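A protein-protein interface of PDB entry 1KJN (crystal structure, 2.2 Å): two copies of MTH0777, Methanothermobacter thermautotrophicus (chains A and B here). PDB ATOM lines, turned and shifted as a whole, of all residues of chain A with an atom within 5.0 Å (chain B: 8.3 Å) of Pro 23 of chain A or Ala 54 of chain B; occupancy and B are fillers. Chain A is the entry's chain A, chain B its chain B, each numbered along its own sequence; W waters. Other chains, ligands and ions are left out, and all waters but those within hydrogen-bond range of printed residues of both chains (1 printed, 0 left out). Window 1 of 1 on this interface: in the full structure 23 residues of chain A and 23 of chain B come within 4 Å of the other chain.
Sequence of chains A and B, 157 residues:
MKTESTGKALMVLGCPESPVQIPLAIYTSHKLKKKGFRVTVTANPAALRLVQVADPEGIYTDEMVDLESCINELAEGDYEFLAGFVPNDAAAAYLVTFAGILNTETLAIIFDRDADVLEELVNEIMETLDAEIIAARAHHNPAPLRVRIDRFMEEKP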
ATOM      1  N   PRO A  19       6.506  23.964  33.858  1.00  0.00           N
ATOM      2  CA  PRO A  19       7.772  24.662  33.654  1.00  0.00           C
ATOM      3  C   PRO A  19       8.201  24.826  32.201  1.00  0.00           C
ATOM      4  O   PRO A  19       9.105  25.623  31.923  1.00  0.00           O
ATOM      5  CB  PRO A  19       8.767  23.840  34.473  1.00  0.00           C
ATOM      6  CG  PRO A  19       8.084  22.499  34.643  1.00  0.00           C
ATOM      7  CD  PRO A  19       6.647  22.847  34.806  1.00  0.00           C
ATOM      8  N   VAL A  20       7.548  24.128  31.265  1.00  0.00           N
ATOM      9  CA  VAL A  20       7.941  24.294  29.862  1.00  0.00           C
ATOM     10  C   VAL A  20       7.349  25.524  29.192  1.00  0.00           C
ATOM     11  O   VAL A  20       7.917  26.006  28.202  1.00  0.00           O
ATOM     12  CB  VAL A  20       7.562  23.089  28.946  1.00  0.00           C
ATOM     13  CG1 VAL A  20       8.241  21.806  29.408  1.00  0.00           C
ATOM     14  CG2 VAL A  20       6.034  22.944  28.833  1.00  0.00           C
ATOM     15  N   GLN A  21       6.277  26.086  29.763  1.00  0.00           N
ATOM     16  CA  GLN A  21       5.606  27.211  29.103  1.00  0.00           C
ATOM     17  C   GLN A  21       6.387  28.483  28.860  1.00  0.00           C
ATOM     18  O   GLN A  21       6.605  28.855  27.711  1.00  0.00           O
ATOM     19  CB  GLN A  21       4.261  27.542  29.744  1.00  0.00           C
ATOM     20  CG  GLN A  21       3.403  28.406  28.832  1.00  0.00           C
ATOM     21  CD  GLN A  21       2.036  28.729  29.420  1.00  0.00           C
ATOM     22  OE1 GLN A  21       1.124  29.128  28.698  1.00  0.00           O
ATOM     23  NE2 GLN A  21       1.891  28.572  30.736  1.00  0.00           N
ATOM     24  N   ILE A  22       6.802  29.166  29.920  1.00  0.00           N
ATOM     25  CA  ILE A  22       7.555  30.406  29.746  1.00  0.00           C
ATOM     26  C   ILE A  22       8.775  30.195  28.836  1.00  0.00           C
ATOM     27  O   ILE A  22       8.922  30.895  27.841  1.00  0.00           O
ATOM     28  CB  ILE A  22       7.978  31.018  31.106  1.00  0.00           C
ATOM     29  CG1 ILE A  22       6.727  31.248  31.945  1.00  0.00           C
ATOM     30  CG2 ILE A  22       8.760  32.319  30.907  1.00  0.00           C
ATOM     31  CD1 ILE A  22       5.625  31.974  31.218  1.00  0.00           C
ATOM     32  N   PRO A  23       9.607  29.176  29.120  1.00  0.00           N
ATOM     33  CA  PRO A  23      10.781  28.955  28.260  1.00  0.00           C
ATOM     34  C   PRO A  23      10.432  28.798  26.774  1.00  0.00           C
ATOM     35  O   PRO A  23      11.050  29.427  25.922  1.00  0.00           O
ATOM     36  CB  PRO A  23      11.384  27.676  28.830  1.00  0.00           C
ATOM     37  CG  PRO A  23      11.145  27.855  30.319  1.00  0.00           C
ATOM     38  CD  PRO A  23       9.662  28.306  30.313  1.00  0.00           C
ATOM     39  N   LEU A  24       9.429  27.980  26.477  1.00  0.00           N
ATOM     40  CA  LEU A  24       8.999  27.763  25.094  1.00  0.00           C
ATOM     41  C   LEU A  24       8.359  29.007  24.466  1.00  0.00           C
ATOM     42  O   LEU A  24       8.441  29.215  23.257  1.00  0.00           O
ATOM     43  CB  LEU A  24       8.035  26.590  25.029  1.00  0.00           C
ATOM     44  CG  LEU A  24       8.692  25.220  25.141  1.00  0.00           C
ATOM     45  CD1 LEU A  24       7.604  24.168  25.236  1.00  0.00           C
ATOM     46  CD2 LEU A  24       9.641  24.972  23.946  1.00  0.00           C
ATOM     47  N   ALA A  25       7.707  29.821  25.282  1.00  0.00           N
ATOM     48  CA  ALA A  25       7.088  31.053  24.792  1.00  0.00           C
ATOM     49  C   ALA A  25       8.214  31.962  24.291  1.00  0.00           C
ATOM     50  O   ALA A  25       8.154  32.509  23.187  1.00  0.00           O
ATOM     51  CB  ALA A  25       6.312  31.739  25.923  1.00  0.00           C
ATOM     52  N   ILE A  26       9.277  32.041  25.084  1.00  0.00           N
ATOM     53  CA  ILE A  26      10.415  32.870  24.737  1.00  0.00           C
ATOM     54  C   ILE A  26      11.127  32.282  23.513  1.00  0.00           C
ATOM     55  O   ILE A  26      11.592  33.028  22.655  1.00  0.00           O
ATOM     56  CB  ILE A  26      11.407  32.973  25.938  1.00  0.00           C
ATOM     57  CG1 ILE A  26      10.744  33.680  27.127  1.00  0.00           C
ATOM     58  CG2 ILE A  26      12.684  33.697  25.531  1.00  0.00           C
ATOM     59  CD1 ILE A  26      11.659  33.773  28.349  1.00  0.00           C
ATOM     60  N   TYR A  27      11.226  30.950  23.455  1.00  0.00           N
ATOM     61  CA  TYR A  27      11.871  30.264  22.336  1.00  0.00           C
ATOM     62  C   TYR A  27      11.117  30.541  21.025  1.00  0.00           C
ATOM     63  O   TYR A  27      11.722  30.849  20.007  1.00  0.00           O
ATOM     64  CB  TYR A  27      11.921  28.750  22.579  1.00  0.00           C
ATOM     65  CG  TYR A  27      12.642  27.995  21.478  1.00  0.00           C
ATOM     66  CD1 TYR A  27      11.932  27.384  20.436  1.00  0.00           C
ATOM     67  CD2 TYR A  27      14.037  27.917  21.457  1.00  0.00           C
ATOM     68  CE1 TYR A  27      12.607  26.713  19.387  1.00  0.00           C
ATOM     69  CE2 TYR A  27      14.718  27.245  20.427  1.00  0.00           C
ATOM     70  CZ  TYR A  27      14.003  26.649  19.398  1.00  0.00           C
ATOM     71  OH  TYR A  27      14.672  25.962  18.414  1.00  0.00           O
ATOM     72  N   ALA A  54      12.982  35.942  33.056  1.00  0.00           N
ATOM     73  CA  ALA A  54      13.735  34.991  32.220  1.00  0.00           C
ATOM     74  C   ALA A  54      14.486  35.663  31.060  1.00  0.00           C
ATOM     75  O   ALA A  54      15.421  35.089  30.505  1.00  0.00           O
ATOM     76  CB  ALA A  54      12.835  33.879  31.686  1.00  0.00           C
ATOM     77  N   TYR A  60      14.434  38.783  23.640  1.00  0.00           N
ATOM     78  CA  TYR A  60      13.617  37.835  22.874  1.00  0.00           C
ATOM     79  C   TYR A  60      12.141  38.190  22.609  1.00  0.00           C
ATOM     80  O   TYR A  60      11.423  37.444  21.939  1.00  0.00           O
ATOM     81  CB  TYR A  60      13.741  36.462  23.519  1.00  0.00           C
ATOM     82  CG  TYR A  60      15.177  35.979  23.622  1.00  0.00           C
ATOM     83  CD1 TYR A  60      15.935  35.735  22.477  1.00  0.00           C
ATOM     84  CD2 TYR A  60      15.757  35.702  24.861  1.00  0.00           C
ATOM     85  CE1 TYR A  60      17.234  35.211  22.563  1.00  0.00           C
ATOM     86  CE2 TYR A  60      17.067  35.182  24.952  1.00  0.00           C
ATOM     87  CZ  TYR A  60      17.788  34.932  23.801  1.00  0.00           C
ATOM     88  OH  TYR A  60      19.036  34.328  23.880  1.00  0.00           O
ATOM     89  N   PRO B  19       7.470  26.753  38.287  1.00  0.00           N
ATOM     90  CA  PRO B  19       7.641  27.691  37.172  1.00  0.00           C
ATOM     91  C   PRO B  19       8.645  28.814  37.442  1.00  0.00           C
ATOM     92  O   PRO B  19       9.186  29.383  36.499  1.00  0.00           O
ATOM     93  CB  PRO B  19       6.239  28.264  36.994  1.00  0.00           C
ATOM     94  CG  PRO B  19       5.343  27.168  37.498  1.00  0.00           C
ATOM     95  CD  PRO B  19       6.054  26.659  38.692  1.00  0.00           C
ATOM     96  N   GLN B  21      11.645  28.624  38.955  1.00  0.00           N
ATOM     97  CA  GLN B  21      13.068  28.270  38.973  1.00  0.00           C
ATOM     98  C   GLN B  21      13.972  28.668  37.818  1.00  0.00           C
ATOM     99  O   GLN B  21      14.935  29.416  38.010  1.00  0.00           O
ATOM    100  CB  GLN B  21      13.267  26.794  39.306  1.00  0.00           C
ATOM    101  CG  GLN B  21      14.731  26.443  39.509  1.00  0.00           C
ATOM    102  CD  GLN B  21      14.943  25.029  40.000  1.00  0.00           C
ATOM    103  OE1 GLN B  21      14.095  24.147  39.806  1.00  0.00           O
ATOM    104  NE2 GLN B  21      16.081  24.801  40.664  1.00  0.00           N
ATOM    105  N   ILE B  22      13.707  28.114  36.642  1.00  0.00           N
ATOM    106  CA  ILE B  22      14.505  28.395  35.461  1.00  0.00           C
ATOM    107  C   ILE B  22      14.579  29.892  35.224  1.00  0.00           C
ATOM    108  O   ILE B  22      15.663  30.433  35.033  1.00  0.00           O
ATOM    109  CB  ILE B  22      13.946  27.646  34.218  1.00  0.00           C
ATOM    110  CG1 ILE B  22      13.969  26.150  34.504  1.00  0.00           C
ATOM    111  CG2 ILE B  22      14.718  27.994  32.965  1.00  0.00           C
ATOM    112  CD1 ILE B  22      15.297  25.644  34.983  1.00  0.00           C
ATOM    113  N   PRO B  23      13.431  30.580  35.240  1.00  0.00           N
ATOM    114  CA  PRO B  23      13.457  32.037  35.023  1.00  0.00           C
ATOM    115  C   PRO B  23      14.357  32.766  36.028  1.00  0.00           C
ATOM    116  O   PRO B  23      15.136  33.649  35.649  1.00  0.00           O
ATOM    117  CB  PRO B  23      11.996  32.431  35.202  1.00  0.00           C
ATOM    118  CG  PRO B  23      11.275  31.242  34.567  1.00  0.00           C
ATOM    119  CD  PRO B  23      12.048  30.062  35.182  1.00  0.00           C
ATOM    120  N   ILE B  26      18.103  32.123  35.392  1.00  0.00           N
ATOM    121  CA  ILE B  26      18.618  32.995  34.348  1.00  0.00           C
ATOM    122  C   ILE B  26      18.776  34.429  34.864  1.00  0.00           C
ATOM    123  O   ILE B  26      19.786  35.080  34.602  1.00  0.00           O
ATOM    124  CB  ILE B  26      17.700  32.995  33.121  1.00  0.00           C
ATOM    125  CG1 ILE B  26      17.741  31.614  32.432  1.00  0.00           C
ATOM    126  CG2 ILE B  26      18.167  34.027  32.115  1.00  0.00           C
ATOM    127  CD1 ILE B  26      16.623  31.411  31.406  1.00  0.00           C
ATOM    128  N   ALA B  46      16.399  17.779  31.948  1.00  0.00           N
ATOM    129  CA  ALA B  46      15.280  18.683  31.625  1.00  0.00           C
ATOM    130  C   ALA B  46      15.567  20.142  32.020  1.00  0.00           C
ATOM    131  O   ALA B  46      15.337  21.067  31.234  1.00  0.00           O
ATOM    132  CB  ALA B  46      13.998  18.198  32.280  1.00  0.00           C
ATOM    133  N   ALA B  47      16.124  20.337  33.214  1.00  0.00           N
ATOM    134  CA  ALA B  47      16.433  21.683  33.693  1.00  0.00           C
ATOM    135  C   ALA B  47      17.376  22.407  32.729  1.00  0.00           C
ATOM    136  O   ALA B  47      17.095  23.541  32.339  1.00  0.00           O
ATOM    137  CB  ALA B  47      17.004  21.640  35.129  1.00  0.00           C
ATOM    138  N   LEU B  48      18.472  21.749  32.318  1.00  0.00           N
ATOM    139  CA  LEU B  48      19.400  22.370  31.357  1.00  0.00           C
ATOM    140  C   LEU B  48      18.707  22.680  30.027  1.00  0.00           C
ATOM    141  O   LEU B  48      18.986  23.712  29.385  1.00  0.00           O
ATOM    142  CB  LEU B  48      20.633  21.485  31.115  1.00  0.00           C
ATOM    143  CG  LEU B  48      21.581  21.346  32.331  1.00  0.00           C
ATOM    144  CD1 LEU B  48      22.880  20.664  31.898  1.00  0.00           C
ATOM    145  CD2 LEU B  48      21.892  22.713  32.938  1.00  0.00           C
ATOM    146  N   ARG B  49      17.802  21.796  29.604  1.00  0.00           N
ATOM    147  CA  ARG B  49      17.080  22.018  28.340  1.00  0.00           C
ATOM    148  C   ARG B  49      16.165  23.216  28.446  1.00  0.00           C
ATOM    149  O   ARG B  49      16.050  24.000  27.507  1.00  0.00           O
ATOM    150  CB  ARG B  49      16.254  20.798  27.912  1.00  0.00           C
ATOM    151  CG  ARG B  49      17.069  19.570  27.582  1.00  0.00           C
ATOM    152  CD  ARG B  49      16.227  18.543  26.831  1.00  0.00           C
ATOM    153  NE  ARG B  49      16.153  18.894  25.416  1.00  0.00           N
ATOM    154  CZ  ARG B  49      17.084  18.576  24.513  1.00  0.00           C
ATOM    155  NH1 ARG B  49      18.151  17.876  24.867  1.00  0.00           N
ATOM    156  NH2 ARG B  49      17.006  19.049  23.279  1.00  0.00           N
ATOM    157  N   LEU B  50      15.483  23.338  29.580  1.00  0.00           N
ATOM    158  CA  LEU B  50      14.597  24.474  29.789  1.00  0.00           C
ATOM    159  C   LEU B  50      15.391  25.771  29.716  1.00  0.00           C
ATOM    160  O   LEU B  50      14.906  26.763  29.164  1.00  0.00           O
ATOM    161  CB  LEU B  50      13.884  24.352  31.133  1.00  0.00           C
ATOM    162  CG  LEU B  50      12.737  23.330  31.161  1.00  0.00           C
ATOM    163  CD1 LEU B  50      12.191  23.101  32.576  1.00  0.00           C
ATOM    164  CD2 LEU B  50      11.662  23.798  30.227  1.00  0.00           C
ATOM    165  N   VAL B  51      16.624  25.762  30.234  1.00  0.00           N
ATOM    166  CA  VAL B  51      17.443  26.965  30.204  1.00  0.00           C
ATOM    167  C   VAL B  51      17.827  27.272  28.767  1.00  0.00           C
ATOM    168  O   VAL B  51      17.759  28.412  28.343  1.00  0.00           O
ATOM    169  CB  VAL B  51      18.748  26.822  31.066  1.00  0.00           C
ATOM    170  CG1 VAL B  51      19.662  28.048  30.871  1.00  0.00           C
ATOM    171  CG2 VAL B  51      18.404  26.679  32.549  1.00  0.00           C
ATOM    172  N   GLN B  52      18.204  26.239  28.016  1.00  0.00           N
ATOM    173  CA  GLN B  52      18.628  26.423  26.635  1.00  0.00           C
ATOM    174  C   GLN B  52      17.542  26.980  25.733  1.00  0.00           C
ATOM    175  O   GLN B  52      17.821  27.821  24.889  1.00  0.00           O
ATOM    176  CB  GLN B  52      19.218  25.136  26.070  1.00  0.00           C
ATOM    177  CG  GLN B  52      20.553  24.802  26.702  1.00  0.00           C
ATOM    178  CD  GLN B  52      21.194  23.541  26.154  1.00  0.00           C
ATOM    179  OE1 GLN B  52      21.933  23.585  25.166  1.00  0.00           O
ATOM    180  NE2 GLN B  52      20.942  22.414  26.813  1.00  0.00           N
ATOM    181  N   VAL B  53      16.299  26.572  25.948  1.00  0.00           N
ATOM    182  CA  VAL B  53      15.212  27.098  25.119  1.00  0.00           C
ATOM    183  C   VAL B  53      14.732  28.481  25.582  1.00  0.00           C
ATOM    184  O   VAL B  53      14.246  29.276  24.762  1.00  0.00           O
ATOM    185  CB  VAL B  53      14.021  26.112  25.021  1.00  0.00           C
ATOM    186  CG1 VAL B  53      14.499  24.734  24.523  1.00  0.00           C
ATOM    187  CG2 VAL B  53      13.316  25.997  26.343  1.00  0.00           C
ATOM    188  N   ALA B  54      14.859  28.767  26.880  1.00  0.00           N
ATOM    189  CA  ALA B  54      14.446  30.075  27.424  1.00  0.00           C
ATOM    190  C   ALA B  54      15.443  31.169  27.041  1.00  0.00           C
ATOM    191  O   ALA B  54      15.095  32.340  26.998  1.00  0.00           O
ATOM    192  CB  ALA B  54      14.305  30.012  28.945  1.00  0.00           C
ATOM    193  N   ASP B  55      16.688  30.767  26.783  1.00  0.00           N
ATOM    194  CA  ASP B  55      17.766  31.677  26.382  1.00  0.00           C
ATOM    195  C   ASP B  55      18.424  30.976  25.188  1.00  0.00           C
ATOM    196  O   ASP B  55      19.571  30.546  25.265  1.00  0.00           O
ATOM    197  CB  ASP B  55      18.785  31.824  27.529  1.00  0.00           C
ATOM    198  CG  ASP B  55      19.962  32.742  27.181  1.00  0.00           C
ATOM    199  OD1 ASP B  55      19.885  33.493  26.189  1.00  0.00           O
ATOM    200  OD2 ASP B  55      20.960  32.755  27.941  1.00  0.00           O
ATOM    201  N   PRO B  56      17.717  30.907  24.044  1.00  0.00           N
ATOM    202  CA  PRO B  56      18.237  30.243  22.843  1.00  0.00           C
ATOM    203  C   PRO B  56      19.594  30.680  22.310  1.00  0.00           C
ATOM    204  O   PRO B  56      20.311  29.860  21.745  1.00  0.00           O
ATOM    205  CB  PRO B  56      17.107  30.414  21.833  1.00  0.00           C
ATOM    206  CG  PRO B  56      16.457  31.687  22.265  1.00  0.00           C
ATOM    207  CD  PRO B  56      16.433  31.563  23.763  1.00  0.00           C
ATOM    208  N   GLU B  57      19.952  31.948  22.481  1.00  0.00           N
ATOM    209  CA  GLU B  57      21.258  32.431  22.018  1.00  0.00           C
ATOM    210  C   GLU B  57      22.385  32.378  23.069  1.00  0.00           C
ATOM    211  O   GLU B  57      23.524  32.761  22.785  1.00  0.00           O
ATOM    212  CB  GLU B  57      21.139  33.851  21.438  1.00  0.00           C
ATOM    213  CG  GLU B  57      20.369  33.946  20.108  1.00  0.00           C
ATOM    214  CD  GLU B  57      20.876  32.988  19.031  1.00  0.00           C
ATOM    215  OE1 GLU B  57      22.079  32.647  19.014  1.00  0.00           O
ATOM    216  OE2 GLU B  57      20.061  32.581  18.176  1.00  0.00           O
ATOM    217  N   GLY B  58      22.065  31.950  24.290  1.00  0.00           N
ATOM    218  CA  GLY B  58      23.082  31.846  25.332  1.00  0.00           C
ATOM    219  C   GLY B  58      23.677  33.183  25.733  1.00  0.00           C
ATOM    220  O   GLY B  58      24.895  33.318  25.852  1.00  0.00           O
ATOM    221  N   ILE B  59      22.803  34.164  25.933  1.00  0.00           N
ATOM    222  CA  ILE B  59      23.185  35.515  26.314  1.00  0.00           C
ATOM    223  C   ILE B  59      23.274  35.751  27.832  1.00  0.00           C
ATOM    224  O   ILE B  59      24.048  36.593  28.299  1.00  0.00           O
ATOM    225  CB  ILE B  59      22.196  36.505  25.660  1.00  0.00           C
ATOM    226  CG1 ILE B  59      22.434  36.501  24.142  1.00  0.00           C
ATOM    227  CG2 ILE B  59      22.305  37.888  26.270  1.00  0.00           C
ATOM    228  CD1 ILE B  59      21.305  37.008  23.332  1.00  0.00           C
ATOM    229  N   TYR B  60      22.507  34.989  28.605  1.00  0.00           N
ATOM    230  CA  TYR B  60      22.506  35.134  30.058  1.00  0.00           C
ATOM    231  C   TYR B  60      23.335  34.075  30.794  1.00  0.00           C
ATOM    232  O   TYR B  60      23.495  34.134  32.014  1.00  0.00           O
ATOM    233  CB  TYR B  60      21.069  35.099  30.535  1.00  0.00           C
ATOM    234  CG  TYR B  60      20.242  36.187  29.906  1.00  0.00           C
ATOM    235  CD1 TYR B  60      20.570  37.529  30.102  1.00  0.00           C
ATOM    236  CD2 TYR B  60      19.123  35.889  29.135  1.00  0.00           C
ATOM    237  CE1 TYR B  60      19.802  38.539  29.558  1.00  0.00           C
ATOM    238  CE2 TYR B  60      18.342  36.912  28.576  1.00  0.00           C
ATOM    239  CZ  TYR B  60      18.689  38.234  28.801  1.00  0.00           C
ATOM    240  OH  TYR B  60      17.906  39.269  28.312  1.00  0.00           O
HETATM  241  O   HOH W   1      16.301  34.577  28.001  1.00  0.00           O
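OD1 of Asp 55 of chain B lies within hydrogen-bond range of OH of Tyr 60 of chain A (2.6 Å).
N of Glu 57 of chain B sits at hydrogen-bond distance from OH of Tyr 60 of chain A, 2.9 Å away.
The backbone carbonyl oxygen (O) of Pro 23 of chain A lies close to the backbone carbonyl oxygen (O) of Val 53 of chain B (3.4 Å).
OD1 of Asp 55 of chain B sits at hydrogen-bond distance from N of Gly 58 of chain B, at 3.3 Å.
The backbone NH (N) of Ile 59 of chain B is in hydrogen-bond range of the side-chain carboxylate (OD1) of Asp 55 of chain B, 3.0 Å away.
N of Tyr 60 of chain B sits at hydrogen-bond distance from OD2 of Asp 55 of chain B, 2.8 Å away.
Among the printed residues, pairs that only touch across the chains: Pro 19 of chain A with Leu 50 of chain B (3.6 Å), Val 20 of chain A with Leu 50 of chain B (3.8 Å), Pro 23 of chain A with Leu 50 of chain B (3.7 Å), Pro 23 of chain A with Ala 54 of chain B (3.7 Å), Ile 26 of chain A with Ala 54 of chain B (3.1 Å), Tyr 27 of chain A with Val 53 of chain B (3.2 Å), Tyr 27 of chain A with Pro 56 of chain B (3.98 Å), Ala 54 of chain A with Pro 23 of chain B (3.9 Å), Ala 54 of chain A with Ile 26 of chain B (3.4 Å), Ala 54 of chain A with Tyr 60 of chain B (3.9 Å), Tyr 60 of chain A with Pro 56 of chain B (3.6 Å), Tyr 60 of chain A with Gly 58 of chain B (3.9 Å) and Tyr 60 of chain A with Ile 59 of chain B (3.6 Å).
Pro 23 of chain A touches three residues of chain B.
Of the printed residues of chain A, Ala 54 of chain B touches Pro 23 (3.7 Å) and Ile 26 (3.1 Å).
Of the printed residues of chain A, Gly 58 of chain B touches Tyr 60.
Of the printed residues of chain A, Ile 26 of chain B touches Ala 54.
Of the printed residues of chain A, Asp 55 of chain B touches Tyr 60 (2.6 Å).
Printed residues of chain B within 4 Å of Tyr 60 of chain A: Asp 55 (2.6 Å), Pro 56 (3.6 Å), Glu 57 (2.9 Å), Gly 58 (3.9 Å) and Ile 59 (3.6 Å).
Printed residues of chain A within 4 Å of Val 53 of chain B: Pro 23 and Tyr 27.
Arg 49 of chain B touches none of the printed residues of chain A.
The nearest printed residue of chain A that does not touch Glu 57 of chain B is Tyr 27 of chain A (7.2 Å).
Of the 11 printed residues of chain A, 7 touch a printed residue of chain B.
Printed residues of chain A that touch a printed residue of chain B: Pro 19, Val 20, Pro 23, Ile 26, Tyr 27, Ala 54 and Tyr 60.
Of the 20 printed residues of chain B, 11 touch a printed residue of chain A.
Among the printed residues, no Asp or Glu carboxylate lies within 4 Å of a Lys or Arg side-chain nitrogen of the other chain.
Pro 23 of chain A touches Ala 54 of chain B, and with the chains exchanged Ala 54 of chain A touches Pro 23 of chain B.
Ile 26 of chain A touches Ala 54 of chain B, and with the chains exchanged Ala 54 of chain A touches Ile 26 of chain B.
Ala 54 of chain A touches Tyr 60 of chain B, but with the chains exchanged Tyr 60 of chain A does not touch Ala 54 of chain B (4.02 Å).
Positions printed for both chains: 19, 21, 22, 23, 26, 54 and 60.
Water W1 lies within hydrogen-bond range of the backbone carbonyl oxygen of Ala 54 of chain A and the backbone carbonyl oxygen of Ala 54 of chain B.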
